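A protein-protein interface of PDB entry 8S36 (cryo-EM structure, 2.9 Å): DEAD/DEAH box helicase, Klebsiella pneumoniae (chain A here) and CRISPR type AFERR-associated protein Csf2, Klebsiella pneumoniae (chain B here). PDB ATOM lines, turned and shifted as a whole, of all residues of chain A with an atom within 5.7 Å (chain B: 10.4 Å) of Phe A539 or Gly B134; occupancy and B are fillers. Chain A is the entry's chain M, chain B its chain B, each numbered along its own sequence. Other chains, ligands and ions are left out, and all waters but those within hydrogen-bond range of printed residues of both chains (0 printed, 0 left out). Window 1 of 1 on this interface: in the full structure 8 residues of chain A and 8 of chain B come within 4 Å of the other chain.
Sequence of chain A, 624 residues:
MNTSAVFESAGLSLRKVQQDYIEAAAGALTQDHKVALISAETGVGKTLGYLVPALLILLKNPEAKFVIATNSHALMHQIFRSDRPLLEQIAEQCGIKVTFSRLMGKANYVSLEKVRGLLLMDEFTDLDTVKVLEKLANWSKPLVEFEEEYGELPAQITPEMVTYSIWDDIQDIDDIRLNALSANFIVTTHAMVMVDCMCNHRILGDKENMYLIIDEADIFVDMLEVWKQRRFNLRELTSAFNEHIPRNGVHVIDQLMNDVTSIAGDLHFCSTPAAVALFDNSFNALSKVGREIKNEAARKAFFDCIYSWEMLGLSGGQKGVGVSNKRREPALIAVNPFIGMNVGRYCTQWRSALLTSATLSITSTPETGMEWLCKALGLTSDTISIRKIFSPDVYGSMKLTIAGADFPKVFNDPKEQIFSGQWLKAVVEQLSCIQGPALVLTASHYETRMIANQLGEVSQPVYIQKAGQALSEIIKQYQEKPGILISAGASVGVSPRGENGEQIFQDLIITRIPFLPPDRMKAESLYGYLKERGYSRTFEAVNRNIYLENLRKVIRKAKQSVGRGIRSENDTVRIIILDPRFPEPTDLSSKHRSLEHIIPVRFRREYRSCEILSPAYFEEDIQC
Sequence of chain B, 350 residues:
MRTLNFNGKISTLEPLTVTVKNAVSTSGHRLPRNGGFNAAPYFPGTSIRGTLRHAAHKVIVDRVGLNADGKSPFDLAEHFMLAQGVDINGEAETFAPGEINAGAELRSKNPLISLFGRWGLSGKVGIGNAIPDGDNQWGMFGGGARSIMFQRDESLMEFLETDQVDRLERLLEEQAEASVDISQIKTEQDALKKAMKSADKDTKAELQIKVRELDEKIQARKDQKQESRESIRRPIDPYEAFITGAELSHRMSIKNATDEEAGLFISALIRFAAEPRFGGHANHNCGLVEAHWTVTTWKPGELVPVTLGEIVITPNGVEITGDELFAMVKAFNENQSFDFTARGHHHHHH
OH of Tyr A527 is in hydrogen-bond range of OD1 of Asp B133, 2.6 Å away.
N of Asp B133 sits at hydrogen-bond distance from O of Glu B247 (2.6 Å).
The side-chain carboxylate of Asp B133 sits at hydrogen-bond distance from the side-chain hydroxyl of Ser B249 (2.5 Å).
OG1 of Thr A538 lies within hydrogen-bond range of N of Ala A541.
The backbone carbonyl oxygen (O) of Ala B40 lies close to the backbone NH (N) of Asn B34, 3.2 Å away.
O of Ile B131 is in hydrogen-bond range of N of Ser B249, at 2.7 Å.
NZ of Lys B9 lies within salt-bridge range of OD2 of Asp B133 (3.3 Å).
Glu A524 touches Asp B135.
Tyr A527 touches Pro B132.
N of Gly B134 touches CE2 of Tyr A527, 3.2 Å away.
CG2 of Thr A538 touches CG2 of Ile B131, 3.9 Å away.
Gly B134 touches Phe A539.
CE2 of Phe A539 touches CB of Asp B135, 3.4 Å away.
Glu A540 touches Ala B40.
Asn A543 touches Asp B135.
No residue of chain B comes within 4 Å of Ala A523.
Of chain B, only Gly B134 (3.6 Å) and Asp B135 (3.4 Å) come within 4 Å of Phe A539.
Glu A540 touches one residue of chain B.
No residue of chain B comes within 4 Å of Val A542.
Ala B39 touches none of the printed residues of chain A.
Printed residues of chain A within 4 Å of Ala B40: Glu A540 (3.2 Å).
Gly B134 touches two residues of chain A.
Of the printed residues of chain A, Asp B135 touches Glu A524 (3.9 Å), Phe A539 (3.4 Å) and Asn A543 (3.99 Å).
Gly B245 touches none of the printed residues of chain A.
The nearest residue of chain B that does not touch Phe A539 is Pro B132 (4.7 Å).
The nearest residue of chain A that does not touch Gly B134 is Glu A524 (5.4 Å).
Of the 24 printed residues of chain B, 6 touch a printed residue of chain A.
Hydrophobic or aromatic side chains of chain B within 4 Å of the printed part of chain A: Ala B40 and Ile B131.
Hydrophobic or aromatic side chains of chain A that line the printed part of chain B: Tyr A527 and Phe A539.
Among the printed residues, 9 pairs touch across the chains.
Among the printed residues, no Asp or Glu carboxylate lies within 4 Å of a Lys or Arg side-chain nitrogen of the other chain.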
ATOM      1  N   ARG A 520      40.186   7.521  -1.892  1.00  0.00           N
ATOM      2  CA  ARG A 520      38.878   7.803  -1.318  1.00  0.00           C
ATOM      3  C   ARG A 520      38.370   9.170  -1.747  1.00  0.00           C
ATOM      4  O   ARG A 520      37.159   9.367  -1.874  1.00  0.00           O
ATOM      5  CB  ARG A 520      38.952   7.717   0.205  1.00  0.00           C
ATOM      6  CG  ARG A 520      39.475   6.382   0.715  1.00  0.00           C
ATOM      7  CD  ARG A 520      39.202   6.181   2.198  1.00  0.00           C
ATOM      8  NE  ARG A 520      39.211   7.435   2.944  1.00  0.00           N
ATOM      9  CZ  ARG A 520      40.297   8.154   3.195  1.00  0.00           C
ATOM     10  NH1 ARG A 520      41.495   7.770   2.782  1.00  0.00           N
ATOM     11  NH2 ARG A 520      40.180   9.287   3.880  1.00  0.00           N
ATOM     12  N   ALA A 523      36.643   8.640  -4.965  1.00  0.00           N
ATOM     13  CA  ALA A 523      35.424   7.866  -4.780  1.00  0.00           C
ATOM     14  C   ALA A 523      34.308   8.740  -4.225  1.00  0.00           C
ATOM     15  O   ALA A 523      33.193   8.758  -4.760  1.00  0.00           O
ATOM     16  CB  ALA A 523      35.696   6.675  -3.863  1.00  0.00           C
ATOM     17  N   GLU A 524      34.603   9.503  -3.172  1.00  0.00           N
ATOM     18  CA  GLU A 524      33.571  10.317  -2.545  1.00  0.00           C
ATOM     19  C   GLU A 524      33.164  11.479  -3.435  1.00  0.00           C
ATOM     20  O   GLU A 524      31.985  11.842  -3.473  1.00  0.00           O
ATOM     21  CB  GLU A 524      34.052  10.847  -1.193  1.00  0.00           C
ATOM     22  CG  GLU A 524      33.902   9.878  -0.027  1.00  0.00           C
ATOM     23  CD  GLU A 524      34.838   8.690  -0.119  1.00  0.00           C
ATOM     24  OE1 GLU A 524      34.924   8.082  -1.204  1.00  0.00           O
ATOM     25  OE2 GLU A 524      35.493   8.369   0.895  1.00  0.00           O
ATOM     26  N   TYR A 527      30.973   9.932  -6.211  1.00  0.00           N
ATOM     27  CA  TYR A 527      29.688   9.602  -5.604  1.00  0.00           C
ATOM     28  C   TYR A 527      28.859  10.854  -5.349  1.00  0.00           C
ATOM     29  O   TYR A 527      27.641  10.854  -5.554  1.00  0.00           O
ATOM     30  CB  TYR A 527      29.912   8.831  -4.303  1.00  0.00           C
ATOM     31  CG  TYR A 527      28.681   8.130  -3.782  1.00  0.00           C
ATOM     32  CD1 TYR A 527      27.983   7.228  -4.571  1.00  0.00           C
ATOM     33  CD2 TYR A 527      28.219   8.368  -2.498  1.00  0.00           C
ATOM     34  CE1 TYR A 527      26.859   6.587  -4.099  1.00  0.00           C
ATOM     35  CE2 TYR A 527      27.096   7.732  -2.017  1.00  0.00           C
ATOM     36  CZ  TYR A 527      26.421   6.840  -2.821  1.00  0.00           C
ATOM     37  OH  TYR A 527      25.298   6.201  -2.349  1.00  0.00           O
ATOM     38  N   ARG A 537      23.368   4.877  -8.322  1.00  0.00           N
ATOM     39  CA  ARG A 537      24.430   3.887  -8.226  1.00  0.00           C
ATOM     40  C   ARG A 537      24.963   3.885  -6.803  1.00  0.00           C
ATOM     41  O   ARG A 537      25.126   4.947  -6.194  1.00  0.00           O
ATOM     42  CB  ARG A 537      25.576   4.172  -9.214  1.00  0.00           C
ATOM     43  CG  ARG A 537      25.157   4.679 -10.599  1.00  0.00           C
ATOM     44  CD  ARG A 537      25.084   3.548 -11.612  1.00  0.00           C
ATOM     45  NE  ARG A 537      26.401   3.010 -11.933  1.00  0.00           N
ATOM     46  CZ  ARG A 537      27.319   3.642 -12.652  1.00  0.00           C
ATOM     47  NH1 ARG A 537      27.100   4.849 -13.153  1.00  0.00           N
ATOM     48  NH2 ARG A 537      28.487   3.049 -12.878  1.00  0.00           N
ATOM     49  N   THR A 538      25.232   2.697  -6.271  1.00  0.00           N
ATOM     50  CA  THR A 538      25.764   2.616  -4.921  1.00  0.00           C
ATOM     51  C   THR A 538      27.203   3.115  -4.891  1.00  0.00           C
ATOM     52  O   THR A 538      27.889   3.186  -5.915  1.00  0.00           O
ATOM     53  CB  THR A 538      25.712   1.181  -4.398  1.00  0.00           C
ATOM     54  OG1 THR A 538      26.619   0.363  -5.148  1.00  0.00           O
ATOM     55  CG2 THR A 538      24.308   0.615  -4.513  1.00  0.00           C
ATOM     56  N   PHE A 539      27.662   3.466  -3.690  1.00  0.00           N
ATOM     57  CA  PHE A 539      29.050   3.885  -3.536  1.00  0.00           C
ATOM     58  C   PHE A 539      30.001   2.750  -3.886  1.00  0.00           C
ATOM     59  O   PHE A 539      31.091   2.986  -4.417  1.00  0.00           O
ATOM     60  CB  PHE A 539      29.303   4.377  -2.115  1.00  0.00           C
ATOM     61  CG  PHE A 539      30.726   4.772  -1.865  1.00  0.00           C
ATOM     62  CD1 PHE A 539      31.184   6.022  -2.244  1.00  0.00           C
ATOM     63  CD2 PHE A 539      31.609   3.893  -1.265  1.00  0.00           C
ATOM     64  CE1 PHE A 539      32.494   6.390  -2.023  1.00  0.00           C
ATOM     65  CE2 PHE A 539      32.920   4.254  -1.043  1.00  0.00           C
ATOM     66  CZ  PHE A 539      33.362   5.505  -1.424  1.00  0.00           C
ATOM     67  N   GLU A 540      29.615   1.513  -3.574  1.00  0.00           N
ATOM     68  CA  GLU A 540      30.446   0.363  -3.918  1.00  0.00           C
ATOM     69  C   GLU A 540      30.601   0.225  -5.426  1.00  0.00           C
ATOM     70  O   GLU A 540      31.677  -0.136  -5.916  1.00  0.00           O
ATOM     71  CB  GLU A 540      29.858  -0.912  -3.311  1.00  0.00           C
ATOM     72  CG  GLU A 540      30.203  -1.117  -1.839  1.00  0.00           C
ATOM     73  CD  GLU A 540      30.128   0.160  -1.028  1.00  0.00           C
ATOM     74  OE1 GLU A 540      29.114   0.882  -1.143  1.00  0.00           O
ATOM     75  OE2 GLU A 540      31.089   0.452  -0.287  1.00  0.00           O
ATOM     76  N   ALA A 541      29.533   0.492  -6.178  1.00  0.00           N
ATOM     77  CA  ALA A 541      29.638   0.440  -7.632  1.00  0.00           C
ATOM     78  C   ALA A 541      30.625   1.482  -8.142  1.00  0.00           C
ATOM     79  O   ALA A 541      31.413   1.208  -9.055  1.00  0.00           O
ATOM     80  CB  ALA A 541      28.264   0.646  -8.266  1.00  0.00           C
ATOM     81  N   VAL A 542      30.599   2.684  -7.566  1.00  0.00           N
ATOM     82  CA  VAL A 542      31.551   3.713  -7.970  1.00  0.00           C
ATOM     83  C   VAL A 542      32.968   3.316  -7.574  1.00  0.00           C
ATOM     84  O   VAL A 542      33.931   3.594  -8.299  1.00  0.00           O
ATOM     85  CB  VAL A 542      31.155   5.070  -7.364  1.00  0.00           C
ATOM     86  CG1 VAL A 542      32.189   6.127  -7.711  1.00  0.00           C
ATOM     87  CG2 VAL A 542      29.774   5.485  -7.850  1.00  0.00           C
ATOM     88  N   ASN A 543      33.123   2.678  -6.412  1.00  0.00           N
ATOM     89  CA  ASN A 543      34.433   2.178  -6.011  1.00  0.00           C
ATOM     90  C   ASN A 543      34.948   1.149  -7.006  1.00  0.00           C
ATOM     91  O   ASN A 543      36.132   1.147  -7.359  1.00  0.00           O
ATOM     92  CB  ASN A 543      34.360   1.572  -4.609  1.00  0.00           C
ATOM     93  CG  ASN A 543      34.679   2.576  -3.523  1.00  0.00           C
ATOM     94  OD1 ASN A 543      34.471   3.776  -3.692  1.00  0.00           O
ATOM     95  ND2 ASN A 543      35.191   2.089  -2.399  1.00  0.00           N
ATOM     96  N   ARG A 544      34.070   0.270  -7.478  1.00  0.00           N
ATOM     97  CA  ARG A 544      34.491  -0.704  -8.475  1.00  0.00           C
ATOM     98  C   ARG A 544      34.836  -0.025  -9.795  1.00  0.00           C
ATOM     99  O   ARG A 544      35.787  -0.426 -10.472  1.00  0.00           O
ATOM    100  CB  ARG A 544      33.400  -1.752  -8.683  1.00  0.00           C
ATOM    101  CG  ARG A 544      33.565  -2.985  -7.803  1.00  0.00           C
ATOM    102  CD  ARG A 544      32.485  -4.027  -8.058  1.00  0.00           C
ATOM    103  NE  ARG A 544      32.177  -4.178  -9.474  1.00  0.00           N
ATOM    104  CZ  ARG A 544      33.002  -4.698 -10.375  1.00  0.00           C
ATOM    105  NH1 ARG A 544      34.198  -5.154 -10.038  1.00  0.00           N
ATOM    106  NH2 ARG A 544      32.616  -4.762 -11.645  1.00  0.00           N
ATOM    107  N   LYS B   9      15.678   8.329   0.550  1.00  0.00           N
ATOM    108  CA  LYS B   9      16.779   8.189   1.489  1.00  0.00           C
ATOM    109  C   LYS B   9      16.268   8.073   2.917  1.00  0.00           C
ATOM    110  O   LYS B   9      15.323   8.764   3.312  1.00  0.00           O
ATOM    111  CB  LYS B   9      17.737   9.376   1.386  1.00  0.00           C
ATOM    112  CG  LYS B   9      18.876   9.158   0.409  1.00  0.00           C
ATOM    113  CD  LYS B   9      19.354  10.470  -0.190  1.00  0.00           C
ATOM    114  CE  LYS B   9      20.608  10.283  -1.029  1.00  0.00           C
ATOM    115  NZ  LYS B   9      20.497   9.134  -1.972  1.00  0.00           N
ATOM    116  N   ASN B  34      27.100  -6.437   2.196  1.00  0.00           N
ATOM    117  CA  ASN B  34      26.780  -6.453   0.770  1.00  0.00           C
ATOM    118  C   ASN B  34      27.780  -7.348   0.035  1.00  0.00           C
ATOM    119  O   ASN B  34      28.604  -6.904  -0.767  1.00  0.00           O
ATOM    120  CB  ASN B  34      26.776  -5.031   0.221  1.00  0.00           C
ATOM    121  CG  ASN B  34      25.909  -4.877  -1.012  1.00  0.00           C
ATOM    122  OD1 ASN B  34      25.140  -5.769  -1.364  1.00  0.00           O
ATOM    123  ND2 ASN B  34      26.025  -3.732  -1.673  1.00  0.00           N
ATOM    124  N   ASN B  38      34.774  -7.500   3.531  1.00  0.00           N
ATOM    125  CA  ASN B  38      35.153  -6.110   3.275  1.00  0.00           C
ATOM    126  C   ASN B  38      34.201  -5.491   2.250  1.00  0.00           C
ATOM    127  O   ASN B  38      34.574  -5.125   1.136  1.00  0.00           O
ATOM    128  CB  ASN B  38      36.600  -6.038   2.805  1.00  0.00           C
ATOM    129  CG  ASN B  38      37.513  -6.961   3.586  1.00  0.00           C
ATOM    130  OD1 ASN B  38      38.312  -7.697   3.008  1.00  0.00           O
ATOM    131  ND2 ASN B  38      37.401  -6.925   4.909  1.00  0.00           N
ATOM    132  N   ALA B  39      32.941  -5.385   2.662  1.00  0.00           N
ATOM    133  CA  ALA B  39      31.886  -4.789   1.861  1.00  0.00           C
ATOM    134  C   ALA B  39      31.130  -3.781   2.711  1.00  0.00           C
ATOM    135  O   ALA B  39      31.209  -3.793   3.942  1.00  0.00           O
ATOM    136  CB  ALA B  39      30.921  -5.849   1.315  1.00  0.00           C
ATOM    137  N   ALA B  40      30.415  -2.888   2.047  1.00  0.00           N
ATOM    138  CA  ALA B  40      29.577  -1.940   2.766  1.00  0.00           C
ATOM    139  C   ALA B  40      28.405  -2.673   3.406  1.00  0.00           C
ATOM    140  O   ALA B  40      27.629  -3.312   2.686  1.00  0.00           O
ATOM    141  CB  ALA B  40      29.066  -0.855   1.829  1.00  0.00           C
ATOM    142  N   PRO B  41      28.230  -2.624   4.726  1.00  0.00           N
ATOM    143  CA  PRO B  41      27.023  -3.214   5.309  1.00  0.00           C
ATOM    144  C   PRO B  41      25.775  -2.475   4.856  1.00  0.00           C
ATOM    145  O   PRO B  41      25.788  -1.265   4.622  1.00  0.00           O
ATOM    146  CB  PRO B  41      27.243  -3.075   6.820  1.00  0.00           C
ATOM    147  CG  PRO B  41      28.305  -2.049   6.970  1.00  0.00           C
ATOM    148  CD  PRO B  41      29.177  -2.206   5.773  1.00  0.00           C
ATOM    149  N   TYR B  42      24.693  -3.232   4.718  1.00  0.00           N
ATOM    150  CA  TYR B  42      23.386  -2.716   4.353  1.00  0.00           C
ATOM    151  C   TYR B  42      22.397  -3.067   5.453  1.00  0.00           C
ATOM    152  O   TYR B  42      22.515  -4.115   6.092  1.00  0.00           O
ATOM    153  CB  TYR B  42      22.910  -3.311   3.029  1.00  0.00           C
ATOM    154  CG  TYR B  42      22.638  -4.795   3.116  1.00  0.00           C
ATOM    155  CD1 TYR B  42      23.675  -5.715   3.057  1.00  0.00           C
ATOM    156  CD2 TYR B  42      21.348  -5.276   3.270  1.00  0.00           C
ATOM    157  CE1 TYR B  42      23.430  -7.069   3.144  1.00  0.00           C
ATOM    158  CE2 TYR B  42      21.097  -6.629   3.355  1.00  0.00           C
ATOM    159  CZ  TYR B  42      22.140  -7.519   3.294  1.00  0.00           C
ATOM    160  OH  TYR B  42      21.890  -8.868   3.379  1.00  0.00           O
ATOM    161  N   ALA B 130      18.362  -1.087   2.498  1.00  0.00           N
ATOM    162  CA  ALA B 130      18.836   0.284   2.644  1.00  0.00           C
ATOM    163  C   ALA B 130      20.357   0.273   2.544  1.00  0.00           C
ATOM    164  O   ALA B 130      21.043  -0.139   3.484  1.00  0.00           O
ATOM    165  CB  ALA B 130      18.369   0.880   3.968  1.00  0.00           C
ATOM    166  N   ILE B 131      20.878   0.722   1.407  1.00  0.00           N
ATOM    167  CA  ILE B 131      22.316   0.705   1.148  1.00  0.00           C
ATOM    168  C   ILE B 131      22.896   2.049   1.576  1.00  0.00           C
ATOM    169  O   ILE B 131      22.358   3.093   1.183  1.00  0.00           O
ATOM    170  CB  ILE B 131      22.605   0.421  -0.335  1.00  0.00           C
ATOM    171  CG1 ILE B 131      22.151  -0.995  -0.705  1.00  0.00           C
ATOM    172  CG2 ILE B 131      24.083   0.622  -0.654  1.00  0.00           C
ATOM    173  CD1 ILE B 131      23.132  -2.078  -0.313  1.00  0.00           C
ATOM    174  N   PRO B 132      23.977   2.092   2.355  1.00  0.00           N
ATOM    175  CA  PRO B 132      24.502   3.388   2.792  1.00  0.00           C
ATOM    176  C   PRO B 132      25.102   4.174   1.638  1.00  0.00           C
ATOM    177  O   PRO B 132      25.479   3.628   0.600  1.00  0.00           O
ATOM    178  CB  PRO B 132      25.572   3.012   3.823  1.00  0.00           C
ATOM    179  CG  PRO B 132      25.988   1.647   3.443  1.00  0.00           C
ATOM    180  CD  PRO B 132      24.750   0.978   2.932  1.00  0.00           C
ATOM    181  N   ASP B 133      25.185   5.485   1.845  1.00  0.00           N
ATOM    182  CA  ASP B 133      25.744   6.419   0.875  1.00  0.00           C
ATOM    183  C   ASP B 133      27.122   6.852   1.356  1.00  0.00           C
ATOM    184  O   ASP B 133      27.237   7.569   2.356  1.00  0.00           O
ATOM    185  CB  ASP B 133      24.818   7.620   0.696  1.00  0.00           C
ATOM    186  CG  ASP B 133      23.477   7.236   0.108  1.00  0.00           C
ATOM    187  OD1 ASP B 133      23.407   6.204  -0.591  1.00  0.00           O
ATOM    188  OD2 ASP B 133      22.492   7.967   0.343  1.00  0.00           O
ATOM    189  N   GLY B 134      28.163   6.424   0.650  1.00  0.00           N
ATOM    190  CA  GLY B 134      29.509   6.849   0.971  1.00  0.00           C
ATOM    191  C   GLY B 134      30.245   5.837   1.832  1.00  0.00           C
ATOM    192  O   GLY B 134      29.653   5.036   2.559  1.00  0.00           O
ATOM    193  N   ASP B 135      31.572   5.882   1.746  1.00  0.00           N
ATOM    194  CA  ASP B 135      32.396   4.999   2.553  1.00  0.00           C
ATOM    195  C   ASP B 135      32.255   5.360   4.026  1.00  0.00           C
ATOM    196  O   ASP B 135      31.792   6.446   4.386  1.00  0.00           O
ATOM    197  CB  ASP B 135      33.865   5.088   2.142  1.00  0.00           C
ATOM    198  CG  ASP B 135      34.550   3.735   2.125  1.00  0.00           C
ATOM    199  OD1 ASP B 135      34.165   2.861   2.932  1.00  0.00           O
ATOM    200  OD2 ASP B 135      35.473   3.545   1.306  1.00  0.00           O
ATOM    201  N   ASN B 136      32.669   4.430   4.883  1.00  0.00           N
ATOM    202  CA  ASN B 136      32.386   4.538   6.307  1.00  0.00           C
ATOM    203  C   ASN B 136      30.881   4.708   6.479  1.00  0.00           C
ATOM    204  O   ASN B 136      30.112   4.117   5.717  1.00  0.00           O
ATOM    205  CB  ASN B 136      33.176   5.693   6.930  1.00  0.00           C
ATOM    206  CG  ASN B 136      34.669   5.550   6.724  1.00  0.00           C
ATOM    207  OD1 ASN B 136      35.134   4.592   6.106  1.00  0.00           O
ATOM    208  ND2 ASN B 136      35.432   6.504   7.245  1.00  0.00           N
ATOM    209  N   GLN B 137      30.443   5.517   7.444  1.00  0.00           N
ATOM    210  CA  GLN B 137      29.050   5.619   7.869  1.00  0.00           C
ATOM    211  C   GLN B 137      28.586   4.384   8.625  1.00  0.00           C
ATOM    212  O   GLN B 137      27.383   4.230   8.859  1.00  0.00           O
ATOM    213  CB  GLN B 137      28.091   5.881   6.702  1.00  0.00           C
ATOM    214  CG  GLN B 137      28.506   7.030   5.804  1.00  0.00           C
ATOM    215  CD  GLN B 137      27.319   7.802   5.264  1.00  0.00           C
ATOM    216  OE1 GLN B 137      26.209   7.276   5.174  1.00  0.00           O
ATOM    217  NE2 GLN B 137      27.546   9.058   4.900  1.00  0.00           N
ATOM    218  N   TRP B 138      29.502   3.496   9.007  1.00  0.00           N
ATOM    219  CA  TRP B 138      29.216   2.418   9.939  1.00  0.00           C
ATOM    220  C   TRP B 138      30.320   2.369  10.986  1.00  0.00           C
ATOM    221  O   TRP B 138      31.468   2.732  10.719  1.00  0.00           O
ATOM    222  CB  TRP B 138      29.105   1.064   9.233  1.00  0.00           C
ATOM    223  CG  TRP B 138      30.224   0.801   8.291  1.00  0.00           C
ATOM    224  CD1 TRP B 138      31.475   0.360   8.606  1.00  0.00           C
ATOM    225  CD2 TRP B 138      30.201   0.965   6.871  1.00  0.00           C
ATOM    226  NE1 TRP B 138      32.233   0.239   7.467  1.00  0.00           N
ATOM    227  CE2 TRP B 138      31.473   0.604   6.388  1.00  0.00           C
ATOM    228  CE3 TRP B 138      29.225   1.378   5.959  1.00  0.00           C
ATOM    229  CZ2 TRP B 138      31.796   0.646   5.035  1.00  0.00           C
ATOM    230  CZ3 TRP B 138      29.549   1.419   4.616  1.00  0.00           C
ATOM    231  CH2 TRP B 138      30.824   1.058   4.168  1.00  0.00           C
ATOM    232  N   GLY B 139      29.958   1.912  12.180  1.00  0.00           N
ATOM    233  CA  GLY B 139      30.885   1.900  13.296  1.00  0.00           C
ATOM    234  C   GLY B 139      30.421   0.945  14.370  1.00  0.00           C
ATOM    235  O   GLY B 139      29.277   0.487  14.376  1.00  0.00           O
ATOM    236  N   PHE B 242      24.951   1.739  11.487  1.00  0.00           N
ATOM    237  CA  PHE B 242      25.159   2.897  10.630  1.00  0.00           C
ATOM    238  C   PHE B 242      25.159   4.158  11.482  1.00  0.00           C
ATOM    239  O   PHE B 242      24.284   4.340  12.329  1.00  0.00           O
ATOM    240  CB  PHE B 242      24.073   2.974   9.562  1.00  0.00           C
ATOM    241  CG  PHE B 242      24.025   1.775   8.667  1.00  0.00           C
ATOM    242  CD1 PHE B 242      24.877   1.673   7.585  1.00  0.00           C
ATOM    243  CD2 PHE B 242      23.132   0.747   8.911  1.00  0.00           C
ATOM    244  CE1 PHE B 242      24.839   0.572   6.761  1.00  0.00           C
ATOM    245  CE2 PHE B 242      23.089  -0.357   8.088  1.00  0.00           C
ATOM    246  CZ  PHE B 242      23.944  -0.445   7.011  1.00  0.00           C
ATOM    247  N   ILE B 243      26.142   5.031  11.260  1.00  0.00           N
ATOM    248  CA  ILE B 243      26.322   6.160  12.166  1.00  0.00           C
ATOM    249  C   ILE B 243      25.141   7.119  12.061  1.00  0.00           C
ATOM    250  O   ILE B 243      24.354   7.095  11.108  1.00  0.00           O
ATOM    251  CB  ILE B 243      27.654   6.884  11.900  1.00  0.00           C
ATOM    252  CG1 ILE B 243      27.596   7.718  10.611  1.00  0.00           C
ATOM    253  CG2 ILE B 243      28.785   5.874  11.830  1.00  0.00           C
ATOM    254  CD1 ILE B 243      28.893   8.444  10.291  1.00  0.00           C
ATOM    255  N   GLY B 245      23.093  10.244  11.195  1.00  0.00           N
ATOM    256  CA  GLY B 245      23.147  11.050   9.995  1.00  0.00           C
ATOM    257  C   GLY B 245      23.544  10.301   8.746  1.00  0.00           C
ATOM    258  O   GLY B 245      23.707  10.929   7.694  1.00  0.00           O
ATOM    259  N   ALA B 246      23.707   8.983   8.822  1.00  0.00           N
ATOM    260  CA  ALA B 246      24.042   8.206   7.639  1.00  0.00           C
ATOM    261  C   ALA B 246      22.884   8.218   6.651  1.00  0.00           C
ATOM    262  O   ALA B 246      21.716   8.104   7.034  1.00  0.00           O
ATOM    263  CB  ALA B 246      24.387   6.770   8.027  1.00  0.00           C
ATOM    264  N   GLU B 247      23.217   8.353   5.371  1.00  0.00           N
ATOM    265  CA  GLU B 247      22.239   8.384   4.289  1.00  0.00           C
ATOM    266  C   GLU B 247      22.181   7.000   3.655  1.00  0.00           C
ATOM    267  O   GLU B 247      23.155   6.554   3.037  1.00  0.00           O
ATOM    268  CB  GLU B 247      22.612   9.447   3.258  1.00  0.00           C
ATOM    269  CG  GLU B 247      22.402  10.874   3.736  1.00  0.00           C
ATOM    270  CD  GLU B 247      20.941  11.272   3.780  1.00  0.00           C
ATOM    271  OE1 GLU B 247      20.149  10.728   2.983  1.00  0.00           O
ATOM    272  OE2 GLU B 247      20.582  12.128   4.615  1.00  0.00           O
ATOM    273  N   LEU B 248      21.046   6.319   3.806  1.00  0.00           N
ATOM    274  CA  LEU B 248      20.859   4.968   3.288  1.00  0.00           C
ATOM    275  C   LEU B 248      19.823   5.014   2.172  1.00  0.00           C
ATOM    276  O   LEU B 248      18.644   5.280   2.425  1.00  0.00           O
ATOM    277  CB  LEU B 248      20.426   4.014   4.397  1.00  0.00           C
ATOM    278  CG  LEU B 248      21.458   3.751   5.495  1.00  0.00           C
ATOM    279  CD1 LEU B 248      21.326   4.760   6.625  1.00  0.00           C
ATOM    280  CD2 LEU B 248      21.314   2.334   6.023  1.00  0.00           C
ATOM    281  N   SER B 249      20.263   4.779   0.940  1.00  0.00           N
ATOM    282  CA  SER B 249      19.342   4.793  -0.189  1.00  0.00           C
ATOM    283  C   SER B 249      18.399   3.600  -0.100  1.00  0.00           C
ATOM    284  O   SER B 249      18.839   2.457   0.061  1.00  0.00           O
ATOM    285  CB  SER B 249      20.115   4.760  -1.505  1.00  0.00           C
ATOM    286  OG  SER B 249      21.107   5.771  -1.537  1.00  0.00           O
